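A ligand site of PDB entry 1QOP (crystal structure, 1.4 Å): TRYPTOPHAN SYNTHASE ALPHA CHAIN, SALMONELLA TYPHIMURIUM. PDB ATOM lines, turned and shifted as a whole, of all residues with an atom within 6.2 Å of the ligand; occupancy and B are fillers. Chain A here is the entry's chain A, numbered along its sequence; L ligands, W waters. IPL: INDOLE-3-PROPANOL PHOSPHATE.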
ATOM      1  N   PHE A  22      -1.138  27.685  -4.975  1.00  0.00           N
ATOM      2  CA  PHE A  22      -1.625  27.493  -3.628  1.00  0.00           C
ATOM      3  C   PHE A  22      -0.448  27.142  -2.721  1.00  0.00           C
ATOM      4  O   PHE A  22       0.398  26.346  -3.154  1.00  0.00           O
ATOM      5  CB  PHE A  22      -2.643  26.339  -3.524  1.00  0.00           C
ATOM      6  CG  PHE A  22      -2.850  25.872  -2.106  1.00  0.00           C
ATOM      7  CD1 PHE A  22      -1.986  24.964  -1.530  1.00  0.00           C
ATOM      8  CD2 PHE A  22      -3.894  26.371  -1.346  1.00  0.00           C
ATOM      9  CE1 PHE A  22      -2.144  24.561  -0.215  1.00  0.00           C
ATOM     10  CE2 PHE A  22      -4.051  25.959  -0.036  1.00  0.00           C
ATOM     11  CZ  PHE A  22      -3.206  25.043   0.547  1.00  0.00           C
ATOM     12  N   GLU A  49      -3.937  31.423  -3.691  1.00  0.00           N
ATOM     13  CA  GLU A  49      -4.858  30.610  -2.913  1.00  0.00           C
ATOM     14  C   GLU A  49      -3.995  30.209  -1.700  1.00  0.00           C
ATOM     15  O   GLU A  49      -2.906  29.663  -1.858  1.00  0.00           O
ATOM     16  CB  GLU A  49      -5.353  29.371  -3.633  1.00  0.00           C
ATOM     17  CG  GLU A  49      -6.593  28.764  -3.026  1.00  0.00           C
ATOM     18  CD  GLU A  49      -7.816  29.678  -3.052  1.00  0.00           C
ATOM     19  OE1 GLU A  49      -7.976  30.495  -3.979  1.00  0.00           O
ATOM     20  OE2 GLU A  49      -8.634  29.500  -2.135  1.00  0.00           O
ATOM     21  N   ALA A  59      -9.654  17.188   2.898  1.00  0.00           N
ATOM     22  CA  ALA A  59      -9.746  17.261   1.434  1.00  0.00           C
ATOM     23  C   ALA A  59      -8.339  17.305   0.833  1.00  0.00           C
ATOM     24  O   ALA A  59      -8.184  17.507  -0.371  1.00  0.00           O
ATOM     25  CB  ALA A  59     -10.569  18.444   0.954  1.00  0.00           C
ATOM     26  N   ASP A  60      -7.307  17.115   1.654  1.00  0.00           N
ATOM     27  CA  ASP A  60      -5.930  17.187   1.211  1.00  0.00           C
ATOM     28  C   ASP A  60      -5.162  15.868   1.246  1.00  0.00           C
ATOM     29  O   ASP A  60      -5.285  15.081   2.186  1.00  0.00           O
ATOM     30  CB  ASP A  60      -5.152  18.209   2.085  1.00  0.00           C
ATOM     31  CG  ASP A  60      -5.529  19.627   1.715  1.00  0.00           C
ATOM     32  OD1 ASP A  60      -5.219  20.015   0.563  1.00  0.00           O
ATOM     33  OD2 ASP A  60      -6.121  20.340   2.561  1.00  0.00           O
ATOM     34  N   ILE A  64      -0.017  18.262   0.938  1.00  0.00           N
ATOM     35  CA  ILE A  64      -0.538  19.381   1.737  1.00  0.00           C
ATOM     36  C   ILE A  64      -0.758  18.970   3.177  1.00  0.00           C
ATOM     37  O   ILE A  64      -0.579  19.795   4.074  1.00  0.00           O
ATOM     38  CB  ILE A  64      -1.723  20.049   1.033  1.00  0.00           C
ATOM     39  CG1 ILE A  64      -1.195  20.740  -0.232  1.00  0.00           C
ATOM     40  CG2 ILE A  64      -2.406  21.035   1.965  1.00  0.00           C
ATOM     41  CD1 ILE A  64      -2.289  21.118  -1.207  1.00  0.00           C
ATOM     42  N   LEU A 100      -8.247  29.103   1.538  1.00  0.00           N
ATOM     43  CA  LEU A 100      -8.760  27.735   1.489  1.00  0.00           C
ATOM     44  C   LEU A 100      -8.892  27.330   2.955  1.00  0.00           C
ATOM     45  O   LEU A 100      -7.888  27.239   3.662  1.00  0.00           O
ATOM     46  CB  LEU A 100      -7.802  26.805   0.773  1.00  0.00           C
ATOM     47  CG  LEU A 100      -8.273  25.359   0.535  1.00  0.00           C
ATOM     48  CD1 LEU A 100      -8.401  24.588   1.837  1.00  0.00           C
ATOM     49  CD2 LEU A 100      -9.571  25.316  -0.247  1.00  0.00           C
ATOM     50  N   TYR A 102     -11.004  25.227   6.311  1.00  0.00           N
ATOM     51  CA  TYR A 102     -11.842  24.135   6.777  1.00  0.00           C
ATOM     52  C   TYR A 102     -12.892  24.809   7.679  1.00  0.00           C
ATOM     53  O   TYR A 102     -12.602  25.810   8.353  1.00  0.00           O
ATOM     54  CB  TYR A 102     -11.052  23.031   7.446  1.00  0.00           C
ATOM     55  CG  TYR A 102     -10.373  22.192   6.370  1.00  0.00           C
ATOM     56  CD1 TYR A 102     -11.047  21.128   5.784  1.00  0.00           C
ATOM     57  CD2 TYR A 102      -9.093  22.491   5.950  1.00  0.00           C
ATOM     58  CE1 TYR A 102     -10.435  20.385   4.779  1.00  0.00           C
ATOM     59  CE2 TYR A 102      -8.490  21.741   4.953  1.00  0.00           C
ATOM     60  CZ  TYR A 102      -9.168  20.692   4.377  1.00  0.00           C
ATOM     61  OH  TYR A 102      -8.563  19.929   3.383  1.00  0.00           O
ATOM     62  N   LEU A 127     -12.892  29.822   0.240  1.00  0.00           N
ATOM     63  CA  LEU A 127     -13.419  28.539  -0.167  1.00  0.00           C
ATOM     64  C   LEU A 127     -13.387  27.648   1.082  1.00  0.00           C
ATOM     65  O   LEU A 127     -12.302  27.388   1.590  1.00  0.00           O
ATOM     66  CB  LEU A 127     -12.555  27.917  -1.267  1.00  0.00           C
ATOM     67  CG  LEU A 127     -13.145  26.712  -2.023  1.00  0.00           C
ATOM     68  CD1 LEU A 127     -12.181  26.320  -3.126  1.00  0.00           C
ATOM     69  CD2 LEU A 127     -13.469  25.544  -1.111  1.00  0.00           C
ATOM     70  N   ALA A 129     -13.651  24.167   2.329  1.00  0.00           N
ATOM     71  CA  ALA A 129     -13.620  22.872   1.657  1.00  0.00           C
ATOM     72  C   ALA A 129     -14.706  21.888   2.042  1.00  0.00           C
ATOM     73  O   ALA A 129     -15.147  21.143   1.165  1.00  0.00           O
ATOM     74  CB  ALA A 129     -12.237  22.279   1.851  1.00  0.00           C
ATOM     75  N   ILE A 153     -17.108  24.712  -5.003  1.00  0.00           N
ATOM     76  CA  ILE A 153     -16.509  23.689  -5.850  1.00  0.00           C
ATOM     77  C   ILE A 153     -17.559  23.018  -6.703  1.00  0.00           C
ATOM     78  O   ILE A 153     -18.616  22.602  -6.254  1.00  0.00           O
ATOM     79  CB  ILE A 153     -15.853  22.602  -4.969  1.00  0.00           C
ATOM     80  CG1 ILE A 153     -14.614  23.156  -4.261  1.00  0.00           C
ATOM     81  CG2 ILE A 153     -15.503  21.383  -5.812  1.00  0.00           C
ATOM     82  CD1 ILE A 153     -13.850  22.234  -3.352  1.00  0.00           C
ATOM     83  N   TYR A 175     -14.663  27.284  -8.503  1.00  0.00           N
ATOM     84  CA  TYR A 175     -13.604  26.277  -8.390  1.00  0.00           C
ATOM     85  C   TYR A 175     -14.074  25.027  -9.140  1.00  0.00           C
ATOM     86  O   TYR A 175     -15.090  24.444  -8.794  1.00  0.00           O
ATOM     87  CB  TYR A 175     -13.298  25.946  -6.947  1.00  0.00           C
ATOM     88  CG  TYR A 175     -12.141  25.001  -6.799  1.00  0.00           C
ATOM     89  CD1 TYR A 175     -12.298  23.632  -7.055  1.00  0.00           C
ATOM     90  CD2 TYR A 175     -10.900  25.445  -6.438  1.00  0.00           C
ATOM     91  CE1 TYR A 175     -11.233  22.753  -6.934  1.00  0.00           C
ATOM     92  CE2 TYR A 175      -9.808  24.591  -6.327  1.00  0.00           C
ATOM     93  CZ  TYR A 175     -10.000  23.242  -6.570  1.00  0.00           C
ATOM     94  OH  TYR A 175      -8.939  22.380  -6.439  1.00  0.00           O
ATOM     95  N   LEU A 177     -13.297  21.287 -10.100  1.00  0.00           N
ATOM     96  CA  LEU A 177     -12.487  20.124  -9.736  1.00  0.00           C
ATOM     97  C   LEU A 177     -12.069  19.329 -10.968  1.00  0.00           C
ATOM     98  O   LEU A 177     -12.932  19.059 -11.792  1.00  0.00           O
ATOM     99  CB  LEU A 177     -13.398  19.269  -8.867  1.00  0.00           C
ATOM    100  CG  LEU A 177     -12.953  18.487  -7.667  1.00  0.00           C
ATOM    101  CD1 LEU A 177     -11.841  19.132  -6.865  1.00  0.00           C
ATOM    102  CD2 LEU A 177     -14.177  18.204  -6.781  1.00  0.00           C
ATOM    103  N   ARG A 179     -11.018  16.269 -10.875  1.00  0.00           N
ATOM    104  CA  ARG A 179     -11.334  14.881 -10.577  1.00  0.00           C
ATOM    105  C   ARG A 179     -11.831  14.695  -9.145  1.00  0.00           C
ATOM    106  O   ARG A 179     -11.808  15.628  -8.332  1.00  0.00           O
ATOM    107  CB  ARG A 179     -10.019  14.083 -10.682  1.00  0.00           C
ATOM    108  CG  ARG A 179      -8.865  14.663  -9.874  1.00  0.00           C
ATOM    109  CD  ARG A 179      -7.757  13.644  -9.606  1.00  0.00           C
ATOM    110  NE  ARG A 179      -6.601  14.236  -8.955  1.00  0.00           N
ATOM    111  CZ  ARG A 179      -6.534  14.476  -7.639  1.00  0.00           C
ATOM    112  NH1 ARG A 179      -7.571  14.175  -6.863  1.00  0.00           N
ATOM    113  NH2 ARG A 179      -5.463  15.028  -7.093  1.00  0.00           N
ATOM    114  N   VAL A 182      -8.701  13.775  -3.463  1.00  0.00           N
ATOM    115  CA  VAL A 182      -8.153  14.863  -2.672  1.00  0.00           C
ATOM    116  C   VAL A 182      -6.986  15.527  -3.383  1.00  0.00           C
ATOM    117  O   VAL A 182      -6.534  15.058  -4.428  1.00  0.00           O
ATOM    118  CB  VAL A 182      -7.690  14.380  -1.290  1.00  0.00           C
ATOM    119  CG1 VAL A 182      -8.841  13.803  -0.480  1.00  0.00           C
ATOM    120  CG2 VAL A 182      -6.597  13.311  -1.415  1.00  0.00           C
ATOM    121  N   THR A 183      -6.479  16.632  -2.850  1.00  0.00           N
ATOM    122  CA  THR A 183      -5.361  17.315  -3.513  1.00  0.00           C
ATOM    123  C   THR A 183      -4.180  16.360  -3.710  1.00  0.00           C
ATOM    124  O   THR A 183      -3.926  15.478  -2.894  1.00  0.00           O
ATOM    125  CB  THR A 183      -4.870  18.548  -2.726  1.00  0.00           C
ATOM    126  OG1 THR A 183      -4.460  18.165  -1.411  1.00  0.00           O
ATOM    127  CG2 THR A 183      -5.975  19.585  -2.632  1.00  0.00           C
ATOM    128  N   GLY A 184      -3.463  16.575  -4.825  1.00  0.00           N
ATOM    129  CA  GLY A 184      -2.258  15.768  -5.039  1.00  0.00           C
ATOM    130  C   GLY A 184      -1.745  15.920  -6.467  1.00  0.00           C
ATOM    131  O   GLY A 184      -2.512  15.798  -7.415  1.00  0.00           O
ATOM    132  N   ALA A 185      -0.441  16.169  -6.602  1.00  0.00           N
ATOM    133  CA  ALA A 185       0.171  16.337  -7.919  1.00  0.00           C
ATOM    134  C   ALA A 185       0.388  15.010  -8.638  1.00  0.00           C
ATOM    135  O   ALA A 185       0.555  14.996  -9.856  1.00  0.00           O
ATOM    136  CB  ALA A 185       1.498  17.063  -7.729  1.00  0.00           C
ATOM    137  N   ASN A 187      -1.809  12.546  -8.907  1.00  0.00           N
ATOM    138  CA  ASN A 187      -2.998  12.108  -9.627  1.00  0.00           C
ATOM    139  C   ASN A 187      -3.534  13.186 -10.563  1.00  0.00           C
ATOM    140  O   ASN A 187      -4.113  14.162 -10.061  1.00  0.00           O
ATOM    141  CB  ASN A 187      -4.127  11.715  -8.659  1.00  0.00           C
ATOM    142  CG  ASN A 187      -5.015  10.708  -9.369  1.00  0.00           C
ATOM    143  OD1 ASN A 187      -5.825  11.037 -10.229  1.00  0.00           O
ATOM    144  ND2 ASN A 187      -4.821   9.447  -8.994  1.00  0.00           N
ATOM    145  N   GLY A 211      -8.813  23.052 -10.588  1.00  0.00           N
ATOM    146  CA  GLY A 211      -7.859  22.645  -9.580  1.00  0.00           C
ATOM    147  C   GLY A 211      -7.946  21.157  -9.243  1.00  0.00           C
ATOM    148  O   GLY A 211      -9.003  20.533  -9.354  1.00  0.00           O
ATOM    149  N   PHE A 212      -6.838  20.628  -8.758  1.00  0.00           N
ATOM    150  CA  PHE A 212      -6.508  19.288  -8.375  1.00  0.00           C
ATOM    151  C   PHE A 212      -5.604  18.668  -9.464  1.00  0.00           C
ATOM    152  O   PHE A 212      -6.011  18.582 -10.619  1.00  0.00           O
ATOM    153  CB  PHE A 212      -7.664  18.338  -8.074  1.00  0.00           C
ATOM    154  CG  PHE A 212      -8.254  18.392  -6.681  1.00  0.00           C
ATOM    155  CD1 PHE A 212      -8.098  19.493  -5.873  1.00  0.00           C
ATOM    156  CD2 PHE A 212      -8.994  17.323  -6.214  1.00  0.00           C
ATOM    157  CE1 PHE A 212      -8.673  19.533  -4.607  1.00  0.00           C
ATOM    158  CE2 PHE A 212      -9.563  17.333  -4.955  1.00  0.00           C
ATOM    159  CZ  PHE A 212      -9.390  18.446  -4.140  1.00  0.00           C
ATOM    160  N   GLY A 213      -4.398  18.263  -9.081  1.00  0.00           N
ATOM    161  CA  GLY A 213      -3.509  17.581  -9.996  1.00  0.00           C
ATOM    162  C   GLY A 213      -2.824  18.419 -11.047  1.00  0.00           C
ATOM    163  O   GLY A 213      -2.122  17.838 -11.908  1.00  0.00           O
ATOM    164  N   ILE A 214      -2.969  19.736 -11.062  1.00  0.00           N
ATOM    165  CA  ILE A 214      -2.303  20.549 -12.080  1.00  0.00           C
ATOM    166  C   ILE A 214      -0.844  20.707 -11.712  1.00  0.00           C
ATOM    167  O   ILE A 214      -0.563  21.369 -10.705  1.00  0.00           O
ATOM    168  CB  ILE A 214      -2.963  21.943 -12.212  1.00  0.00           C
ATOM    169  CG1 ILE A 214      -4.449  21.794 -12.527  1.00  0.00           C
ATOM    170  CG2 ILE A 214      -2.245  22.808 -13.235  1.00  0.00           C
ATOM    171  CD1 ILE A 214      -4.765  21.277 -13.901  1.00  0.00           C
ATOM    172  N   ILE A 232      -5.327  26.425 -10.872  1.00  0.00           N
ATOM    173  CA  ILE A 232      -4.705  26.490  -9.557  1.00  0.00           C
ATOM    174  C   ILE A 232      -3.770  25.299  -9.390  1.00  0.00           C
ATOM    175  O   ILE A 232      -4.167  24.213  -9.831  1.00  0.00           O
ATOM    176  CB  ILE A 232      -5.786  26.420  -8.452  1.00  0.00           C
ATOM    177  CG1 ILE A 232      -6.635  27.682  -8.485  1.00  0.00           C
ATOM    178  CG2 ILE A 232      -5.145  26.198  -7.091  1.00  0.00           C
ATOM    179  CD1 ILE A 232      -7.959  27.566  -7.753  1.00  0.00           C
ATOM    180  N   SER A 233      -2.582  25.498  -8.827  1.00  0.00           N
ATOM    181  CA  SER A 233      -1.621  24.418  -8.616  1.00  0.00           C
ATOM    182  C   SER A 233      -1.106  24.508  -7.190  1.00  0.00           C
ATOM    183  O   SER A 233      -0.620  25.590  -6.823  1.00  0.00           O
ATOM    184  CB  SER A 233      -0.445  24.569  -9.580  1.00  0.00           C
ATOM    185  OG  SER A 233       0.557  23.592  -9.365  1.00  0.00           O
ATOM    186  N   GLY A 234      -1.316  23.446  -6.404  1.00  0.00           N
ATOM    187  CA  GLY A 234      -0.884  23.500  -5.010  1.00  0.00           C
ATOM    188  C   GLY A 234       0.207  22.497  -4.696  1.00  0.00           C
ATOM    189  O   GLY A 234       1.342  22.901  -4.429  1.00  0.00           O
ATOM    190  N   SER A 235      -0.131  21.217  -4.719  1.00  0.00           N
ATOM    191  CA  SER A 235       0.826  20.159  -4.389  1.00  0.00           C
ATOM    192  C   SER A 235       2.133  20.275  -5.167  1.00  0.00           C
ATOM    193  O   SER A 235       3.198  20.126  -4.555  1.00  0.00           O
ATOM    194  CB  SER A 235       0.182  18.789  -4.565  1.00  0.00           C
ATOM    195  OG  SER A 235      -0.850  18.585  -3.612  1.00  0.00           O
ATOM    196  N   ALA A 236       2.085  20.622  -6.453  1.00  0.00           N
ATOM    197  CA  ALA A 236       3.336  20.757  -7.207  1.00  0.00           C
ATOM    198  C   ALA A 236       4.220  21.862  -6.659  1.00  0.00           C
ATOM    199  O   ALA A 236       5.450  21.760  -6.701  1.00  0.00           O
ATOM    200  CB  ALA A 236       3.015  21.009  -8.662  1.00  0.00           C
HETATM  201  N1  IPL L   1      -6.332  22.365  -0.605  1.00  0.00           N
HETATM  202  C2  IPL L   1      -5.642  23.078  -1.567  1.00  0.00           C
HETATM  203  C3  IPL L   1      -6.459  23.384  -2.628  1.00  0.00           C
HETATM  204  C4  IPL L   1      -8.961  22.792  -2.980  1.00  0.00           C
HETATM  205  C5  IPL L   1     -10.024  22.121  -2.393  1.00  0.00           C
HETATM  206  C6  IPL L   1      -9.887  21.494  -1.161  1.00  0.00           C
HETATM  207  C7  IPL L   1      -8.694  21.497  -0.472  1.00  0.00           C
HETATM  208  C8  IPL L   1      -7.623  22.169  -1.058  1.00  0.00           C
HETATM  209  C9  IPL L   1      -7.730  22.812  -2.304  1.00  0.00           C
HETATM  210  C1' IPL L   1      -4.737  22.247  -4.985  1.00  0.00           C
HETATM  211  C2' IPL L   1      -6.051  22.981  -4.990  1.00  0.00           C
HETATM  212  C3' IPL L   1      -6.125  24.084  -3.907  1.00  0.00           C
HETATM  213  P   IPL L   1      -3.400  20.205  -5.966  1.00  0.00           P
HETATM  214  O1P IPL L   1      -2.648  20.183  -4.672  1.00  0.00           O
HETATM  215  O2P IPL L   1      -2.681  21.021  -7.006  1.00  0.00           O
HETATM  216  O3P IPL L   1      -3.890  18.892  -6.485  1.00  0.00           O
HETATM  217  O4P IPL L   1      -4.793  21.013  -5.712  1.00  0.00           O
HETATM  218  O   HOH W   1      -4.237  21.484  -9.126  1.00  0.00           O
HETATM  219  O   HOH W   2      -0.244  20.254  -8.019  1.00  0.00           O
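Merely in contact with the ligand: Phe 22 (3.6 Å), Ala 59 (3.8 Å), Ile 64 (3.6 Å), Leu 100 (3.6 Å), Ala 129 (3.9 Å), Ile 153 (3.9 Å), Tyr 175 (3.3 Å), Thr 183 (3.4 Å), Phe 212 (3.3 Å), Ile 232 (3.9 Å) and Ser 233 (3.8 Å).
Hydrophobic or aromatic side chains that line the ligand: Phe 22, Ala 59, Ile 64, Leu 100, Ala 129, Ile 153, Tyr 175, Phe 212 and Ile 232.
Of the 27 residues printed, 16 come within 4 Å of the ligand.
An oxygen (O1P) of the ligand is in hydrogen-bond range of the backbone NH of Ser 235, at 2.7 Å.
N of Gly 234 is in hydrogen-bond range of O2P of the ligand (2.8 Å).
The backbone NH (N) of Gly 213 sits at hydrogen-bond distance from an oxygen (O3P) of the ligand, 2.7 Å away.
N1 of the ligand is in hydrogen-bond range of OD1 of Asp 60, at 2.9 Å.
N of Gly 184 lies within hydrogen-bond range of O3P of the ligand.
The side-chain hydroxyl (OG) of Ser 235 sits at hydrogen-bond distance from an oxygen (O1P) of the ligand (2.6 Å).
OH of Tyr 102 is in hydrogen-bond range of OD2 of Asp 60, 2.6 Å away.
OD1 of Asp 60 is in hydrogen-bond range of OG1 of Thr 183, at 2.8 Å.
The backbone carbonyl oxygen (O) of Ala 59 is in hydrogen-bond range of the backbone NH (N) of Thr 183, at 3.1 Å.
The backbone carbonyl oxygen (O) of Ser 233 sits at hydrogen-bond distance from the backbone NH (N) of Phe 22 (2.8 Å).
O of Gly 211 lies close to OH of Tyr 175 (3.5 Å).
The backbone carbonyl oxygen of Ile 214 sits at hydrogen-bond distance from the side-chain hydroxyl of Ser 233 (2.8 Å).
The guanidinium group (NH2) of Arg 179 is in hydrogen-bond range of the backbone carbonyl oxygen (O) of Gly 184 (3.1 Å).
The backbone NH (N) of Ala 59 sits at hydrogen-bond distance from the side-chain hydroxyl (OH) of Tyr 102.
Water W2 lies within hydrogen-bond range of O2P of the ligand (2.7 Å), N of Ala 236 (2.8 Å), O of Ile 214 (2.9 Å) and N of Ser 235 (3.4 Å).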
